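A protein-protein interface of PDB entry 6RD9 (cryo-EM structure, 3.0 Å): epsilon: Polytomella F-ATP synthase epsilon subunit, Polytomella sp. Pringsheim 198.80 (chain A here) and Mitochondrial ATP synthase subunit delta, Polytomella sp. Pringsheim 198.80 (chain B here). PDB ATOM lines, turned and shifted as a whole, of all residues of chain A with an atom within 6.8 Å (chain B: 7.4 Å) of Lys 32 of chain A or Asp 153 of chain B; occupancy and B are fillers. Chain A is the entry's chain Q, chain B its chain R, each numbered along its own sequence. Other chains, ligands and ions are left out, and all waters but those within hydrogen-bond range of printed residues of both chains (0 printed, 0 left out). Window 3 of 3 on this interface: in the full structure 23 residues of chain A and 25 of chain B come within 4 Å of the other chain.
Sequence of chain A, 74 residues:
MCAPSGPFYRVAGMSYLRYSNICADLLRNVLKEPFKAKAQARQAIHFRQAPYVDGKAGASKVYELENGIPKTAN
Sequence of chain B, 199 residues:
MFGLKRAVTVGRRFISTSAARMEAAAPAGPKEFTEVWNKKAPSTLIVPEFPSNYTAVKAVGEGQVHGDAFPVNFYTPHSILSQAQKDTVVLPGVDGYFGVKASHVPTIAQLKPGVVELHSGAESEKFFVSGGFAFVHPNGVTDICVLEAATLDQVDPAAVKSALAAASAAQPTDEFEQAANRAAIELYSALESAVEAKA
Printed residues of chain B within 4 Å of Val 30 of chain A: Val 155 (3.6 Å) and Asp 156 (2.9 Å). Of the printed residues of chain B, Leu 31 of chain A touches Ala 150 (3.7 Å), Gln 154 (3.3 Å) and Asp 156 (3.8 Å). Of chain B, only Asp 153 and Gln 154 come within 4 Å of Lys 32 of chain A. Of the printed residues of chain B, Phe 35 of chain A touches Gln 154. Lys 38 of chain A touches none of the printed residues of chain B. Printed residues of chain A within 4 Å of Ala 150 of chain B: Leu 31 (3.7 Å). Thr 151 of chain B touches none of the printed residues of chain A. Asp 153 of chain B touches one residue of chain A. The nearest residue of chain B that does not touch Lys 32 of chain A is Val 155 of chain B (4.2 Å). The nearest residue of chain A that does not touch Asp 153 of chain B is Phe 35 of chain A (6.2 Å). The nearest printed residue of chain A that does not touch Val 155 of chain B is Lys 32 of chain A (4.2 Å).
The backbone NH (N) of Asp 156 of chain B sits at hydrogen-bond distance from the backbone carbonyl oxygen (O) of Val 30 of chain A, 3.1 Å away. The side-chain amino group of Lys 32 of chain A sits at hydrogen-bond distance from the backbone carbonyl oxygen of Asp 153 of chain B. The backbone NH of Lys 32 of chain A is in hydrogen-bond range of the backbone carbonyl oxygen of Gln 154 of chain B (2.6 Å).
Of the 10 printed residues of chain A, 4 touch a printed residue of chain B. Hydrophobic or aromatic side chains of chain A that line the printed part of chain B: Val 30, Leu 31 and Phe 35. Of the 9 printed residues of chain B, 5 touch a printed residue of chain A. Among the printed residues, 8 pairs touch across the chains.
CG1 of Val 155 of chain B touches O of Val 30 of chain A (3.6 Å). Ala 150 of chain B touches Leu 31 of chain A (CB to CD1, 3.7 Å). Leu 31 of chain A touches Gln 154 of chain B (CA to O, 3.3 Å). Asp 156 of chain B touches Leu 31 of chain A. CD1 of Phe 35 of chain A touches OE1 of Gln 154 of chain B, 3.2 Å away.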
ATOM      1  N   ARG A  28       8.538  -3.430  -0.991  1.00  0.00           N
ATOM      2  CA  ARG A  28       7.546  -4.497  -1.089  1.00  0.00           C
ATOM      3  C   ARG A  28       7.807  -5.420  -2.271  1.00  0.00           C
ATOM      4  O   ARG A  28       7.462  -6.603  -2.212  1.00  0.00           O
ATOM      5  CB  ARG A  28       6.141  -3.907  -1.189  1.00  0.00           C
ATOM      6  CG  ARG A  28       5.715  -3.110   0.025  1.00  0.00           C
ATOM      7  CD  ARG A  28       4.281  -2.655  -0.095  1.00  0.00           C
ATOM      8  NE  ARG A  28       3.987  -1.583   0.844  1.00  0.00           N
ATOM      9  CZ  ARG A  28       3.854  -0.315   0.493  1.00  0.00           C
ATOM     10  NH1 ARG A  28       3.976   0.031  -0.779  1.00  0.00           N
ATOM     11  NH2 ARG A  28       3.597   0.604   1.409  1.00  0.00           N
ATOM     12  N   VAL A  30      10.517  -6.674  -3.075  1.00  0.00           N
ATOM     13  CA  VAL A  30      11.676  -7.473  -2.711  1.00  0.00           C
ATOM     14  C   VAL A  30      11.319  -8.453  -1.582  1.00  0.00           C
ATOM     15  O   VAL A  30      12.139  -9.287  -1.178  1.00  0.00           O
ATOM     16  CB  VAL A  30      12.842  -6.512  -2.368  1.00  0.00           C
ATOM     17  CG1 VAL A  30      14.178  -7.159  -2.063  1.00  0.00           C
ATOM     18  CG2 VAL A  30      13.058  -5.550  -3.515  1.00  0.00           C
ATOM     19  N   LEU A  31      10.065  -8.459  -1.144  1.00  0.00           N
ATOM     20  CA  LEU A  31       9.694  -9.327  -0.039  1.00  0.00           C
ATOM     21  C   LEU A  31       9.516 -10.781  -0.482  1.00  0.00           C
ATOM     22  O   LEU A  31       9.408 -11.104  -1.670  1.00  0.00           O
ATOM     23  CB  LEU A  31       8.416  -8.838   0.637  1.00  0.00           C
ATOM     24  CG  LEU A  31       8.617  -8.211   2.014  1.00  0.00           C
ATOM     25  CD1 LEU A  31       9.431  -6.964   1.880  1.00  0.00           C
ATOM     26  CD2 LEU A  31       7.293  -7.914   2.702  1.00  0.00           C
ATOM     27  N   LYS A  32       9.503 -11.656   0.526  1.00  0.00           N
ATOM     28  CA  LYS A  32       9.162 -13.064   0.369  1.00  0.00           C
ATOM     29  C   LYS A  32       7.726 -13.197  -0.123  1.00  0.00           C
ATOM     30  O   LYS A  32       6.859 -12.416   0.265  1.00  0.00           O
ATOM     31  CB  LYS A  32       9.319 -13.762   1.718  1.00  0.00           C
ATOM     32  CG  LYS A  32       9.089 -15.244   1.742  1.00  0.00           C
ATOM     33  CD  LYS A  32       8.967 -15.735   3.176  1.00  0.00           C
ATOM     34  CE  LYS A  32      10.304 -15.761   3.877  1.00  0.00           C
ATOM     35  NZ  LYS A  32      10.197 -16.227   5.286  1.00  0.00           N
ATOM     36  N   GLU A  33       7.469 -14.201  -0.974  1.00  0.00           N
ATOM     37  CA  GLU A  33       6.170 -14.353  -1.632  1.00  0.00           C
ATOM     38  C   GLU A  33       4.997 -14.724  -0.713  1.00  0.00           C
ATOM     39  O   GLU A  33       3.875 -14.275  -0.986  1.00  0.00           O
ATOM     40  CB  GLU A  33       6.287 -15.356  -2.788  1.00  0.00           C
ATOM     41  CG  GLU A  33       5.102 -15.368  -3.757  1.00  0.00           C
ATOM     42  CD  GLU A  33       4.751 -13.999  -4.339  1.00  0.00           C
ATOM     43  OE1 GLU A  33       3.557 -13.780  -4.631  1.00  0.00           O
ATOM     44  OE2 GLU A  33       5.659 -13.171  -4.574  1.00  0.00           O
ATOM     45  N   PRO A  34       5.169 -15.479   0.384  1.00  0.00           N
ATOM     46  CA  PRO A  34       4.113 -15.489   1.417  1.00  0.00           C
ATOM     47  C   PRO A  34       3.820 -14.133   2.051  1.00  0.00           C
ATOM     48  O   PRO A  34       2.783 -13.993   2.713  1.00  0.00           O
ATOM     49  CB  PRO A  34       4.654 -16.475   2.453  1.00  0.00           C
ATOM     50  CG  PRO A  34       5.362 -17.452   1.638  1.00  0.00           C
ATOM     51  CD  PRO A  34       6.011 -16.686   0.524  1.00  0.00           C
ATOM     52  N   PHE A  35       4.691 -13.139   1.881  1.00  0.00           N
ATOM     53  CA  PHE A  35       4.458 -11.807   2.398  1.00  0.00           C
ATOM     54  C   PHE A  35       4.440 -10.726   1.329  1.00  0.00           C
ATOM     55  O   PHE A  35       4.102  -9.584   1.646  1.00  0.00           O
ATOM     56  CB  PHE A  35       5.520 -11.476   3.449  1.00  0.00           C
ATOM     57  CG  PHE A  35       5.558 -12.458   4.574  1.00  0.00           C
ATOM     58  CD1 PHE A  35       4.676 -12.339   5.637  1.00  0.00           C
ATOM     59  CD2 PHE A  35       6.451 -13.511   4.562  1.00  0.00           C
ATOM     60  CE1 PHE A  35       4.702 -13.248   6.679  1.00  0.00           C
ATOM     61  CE2 PHE A  35       6.486 -14.422   5.589  1.00  0.00           C
ATOM     62  CZ  PHE A  35       5.609 -14.291   6.655  1.00  0.00           C
ATOM     63  N   LYS A  36       4.788 -11.047   0.081  1.00  0.00           N
ATOM     64  CA  LYS A  36       4.828 -10.035  -0.970  1.00  0.00           C
ATOM     65  C   LYS A  36       3.431  -9.687  -1.466  1.00  0.00           C
ATOM     66  O   LYS A  36       3.139  -8.520  -1.751  1.00  0.00           O
ATOM     67  CB  LYS A  36       5.697 -10.519  -2.129  1.00  0.00           C
ATOM     68  CG  LYS A  36       5.883  -9.500  -3.243  1.00  0.00           C
ATOM     69  CD  LYS A  36       6.774 -10.036  -4.347  1.00  0.00           C
ATOM     70  CE  LYS A  36       6.987  -9.005  -5.439  1.00  0.00           C
ATOM     71  NZ  LYS A  36       5.723  -8.709  -6.152  1.00  0.00           N
ATOM     72  N   ALA A  37       2.553 -10.685  -1.581  1.00  0.00           N
ATOM     73  CA  ALA A  37       1.216 -10.435  -2.108  1.00  0.00           C
ATOM     74  C   ALA A  37       0.305  -9.803  -1.070  1.00  0.00           C
ATOM     75  O   ALA A  37      -0.612  -9.062  -1.431  1.00  0.00           O
ATOM     76  CB  ALA A  37       0.598 -11.731  -2.631  1.00  0.00           C
ATOM     77  N   LYS A  38       0.514 -10.099   0.213  1.00  0.00           N
ATOM     78  CA  LYS A  38      -0.277  -9.436   1.244  1.00  0.00           C
ATOM     79  C   LYS A  38       0.191  -8.001   1.442  1.00  0.00           C
ATOM     80  O   LYS A  38      -0.567  -7.146   1.910  1.00  0.00           O
ATOM     81  CB  LYS A  38      -0.215 -10.225   2.552  1.00  0.00           C
ATOM     82  CG  LYS A  38       1.158 -10.283   3.191  1.00  0.00           C
ATOM     83  CD  LYS A  38       1.153 -11.104   4.462  1.00  0.00           C
ATOM     84  CE  LYS A  38       0.348 -10.417   5.548  1.00  0.00           C
ATOM     85  NZ  LYS A  38       0.961  -9.135   5.959  1.00  0.00           N
ATOM     86  N   LYS B 126      15.700  -7.591  14.019  1.00  0.00           N
ATOM     87  CA  LYS B 126      16.257  -6.688  13.017  1.00  0.00           C
ATOM     88  C   LYS B 126      15.231  -6.443  11.920  1.00  0.00           C
ATOM     89  O   LYS B 126      15.013  -7.300  11.061  1.00  0.00           O
ATOM     90  CB  LYS B 126      17.544  -7.255  12.436  1.00  0.00           C
ATOM     91  CG  LYS B 126      18.665  -7.416  13.444  1.00  0.00           C
ATOM     92  CD  LYS B 126      19.936  -7.914  12.774  1.00  0.00           C
ATOM     93  CE  LYS B 126      21.005  -8.258  13.794  1.00  0.00           C
ATOM     94  NZ  LYS B 126      21.541  -7.068  14.499  1.00  0.00           N
ATOM     95  N   ALA B 150       9.932  -4.124   6.915  1.00  0.00           N
ATOM     96  CA  ALA B 150      10.035  -5.557   6.720  1.00  0.00           C
ATOM     97  C   ALA B 150      11.154  -6.120   7.577  1.00  0.00           C
ATOM     98  O   ALA B 150      12.244  -5.549   7.634  1.00  0.00           O
ATOM     99  CB  ALA B 150      10.303  -5.876   5.254  1.00  0.00           C
ATOM    100  N   THR B 151      10.882  -7.224   8.254  1.00  0.00           N
ATOM    101  CA  THR B 151      11.970  -7.994   8.826  1.00  0.00           C
ATOM    102  C   THR B 151      12.743  -8.653   7.690  1.00  0.00           C
ATOM    103  O   THR B 151      12.188  -8.973   6.639  1.00  0.00           O
ATOM    104  CB  THR B 151      11.433  -9.037   9.808  1.00  0.00           C
ATOM    105  OG1 THR B 151      10.385  -8.451  10.581  1.00  0.00           O
ATOM    106  CG2 THR B 151      12.505  -9.487  10.775  1.00  0.00           C
ATOM    107  N   LEU B 152      14.045  -8.833   7.896  1.00  0.00           N
ATOM    108  CA  LEU B 152      14.908  -9.414   6.875  1.00  0.00           C
ATOM    109  C   LEU B 152      14.659 -10.897   6.651  1.00  0.00           C
ATOM    110  O   LEU B 152      15.169 -11.450   5.671  1.00  0.00           O
ATOM    111  CB  LEU B 152      16.360  -9.179   7.265  1.00  0.00           C
ATOM    112  CG  LEU B 152      16.795  -7.742   7.002  1.00  0.00           C
ATOM    113  CD1 LEU B 152      18.046  -7.443   7.763  1.00  0.00           C
ATOM    114  CD2 LEU B 152      17.016  -7.540   5.510  1.00  0.00           C
ATOM    115  N   ASP B 153      13.886 -11.545   7.528  1.00  0.00           N
ATOM    116  CA  ASP B 153      13.539 -12.944   7.336  1.00  0.00           C
ATOM    117  C   ASP B 153      12.619 -13.125   6.142  1.00  0.00           C
ATOM    118  O   ASP B 153      12.660 -14.169   5.485  1.00  0.00           O
ATOM    119  CB  ASP B 153      12.868 -13.482   8.595  1.00  0.00           C
ATOM    120  CG  ASP B 153      13.755 -13.366   9.811  1.00  0.00           C
ATOM    121  OD1 ASP B 153      14.990 -13.349   9.637  1.00  0.00           O
ATOM    122  OD2 ASP B 153      13.219 -13.286  10.937  1.00  0.00           O
ATOM    123  N   GLN B 154      11.811 -12.111   5.828  1.00  0.00           N
ATOM    124  CA  GLN B 154      10.864 -12.165   4.725  1.00  0.00           C
ATOM    125  C   GLN B 154      11.306 -11.328   3.533  1.00  0.00           C
ATOM    126  O   GLN B 154      10.465 -10.874   2.755  1.00  0.00           O
ATOM    127  CB  GLN B 154       9.474 -11.745   5.203  1.00  0.00           C
ATOM    128  CG  GLN B 154       9.355 -10.346   5.752  1.00  0.00           C
ATOM    129  CD  GLN B 154       8.012 -10.100   6.398  1.00  0.00           C
ATOM    130  OE1 GLN B 154       7.344 -11.032   6.837  1.00  0.00           O
ATOM    131  NE2 GLN B 154       7.608  -8.840   6.458  1.00  0.00           N
ATOM    132  N   VAL B 155      12.593 -11.108   3.380  1.00  0.00           N
ATOM    133  CA  VAL B 155      13.148 -10.478   2.190  1.00  0.00           C
ATOM    134  C   VAL B 155      13.946 -11.530   1.432  1.00  0.00           C
ATOM    135  O   VAL B 155      14.627 -12.361   2.044  1.00  0.00           O
ATOM    136  CB  VAL B 155      14.016  -9.261   2.580  1.00  0.00           C
ATOM    137  CG1 VAL B 155      14.522  -8.527   1.355  1.00  0.00           C
ATOM    138  CG2 VAL B 155      13.238  -8.323   3.486  1.00  0.00           C
ATOM    139  N   ASP B 156      13.840 -11.532   0.089  1.00  0.00           N
ATOM    140  CA  ASP B 156      14.781 -12.487  -0.491  1.00  0.00           C
ATOM    141  C   ASP B 156      15.964 -11.777  -1.143  1.00  0.00           C
ATOM    142  O   ASP B 156      15.794 -10.733  -1.784  1.00  0.00           O
ATOM    143  CB  ASP B 156      14.105 -13.417  -1.507  1.00  0.00           C
ATOM    144  CG  ASP B 156      13.114 -12.710  -2.421  1.00  0.00           C
ATOM    145  OD1 ASP B 156      13.255 -11.505  -2.699  1.00  0.00           O
ATOM    146  OD2 ASP B 156      12.179 -13.393  -2.883  1.00  0.00           O
ATOM    147  N   LYS B 198      24.471 -11.445   8.394  1.00  0.00           N
ATOM    148  CA  LYS B 198      23.496 -11.984   9.330  1.00  0.00           C
ATOM    149  C   LYS B 198      24.106 -13.137  10.118  1.00  0.00           C
ATOM    150  O   LYS B 198      24.944 -13.882   9.598  1.00  0.00           O
ATOM    151  CB  LYS B 198      22.239 -12.442   8.585  1.00  0.00           C
ATOM    152  CG  LYS B 198      21.577 -11.380   7.687  1.00  0.00           C
ATOM    153  CD  LYS B 198      20.929 -10.217   8.453  1.00  0.00           C
ATOM    154  CE  LYS B 198      21.763  -8.933   8.404  1.00  0.00           C
ATOM    155  NZ  LYS B 198      21.107  -7.813   9.125  1.00  0.00           N
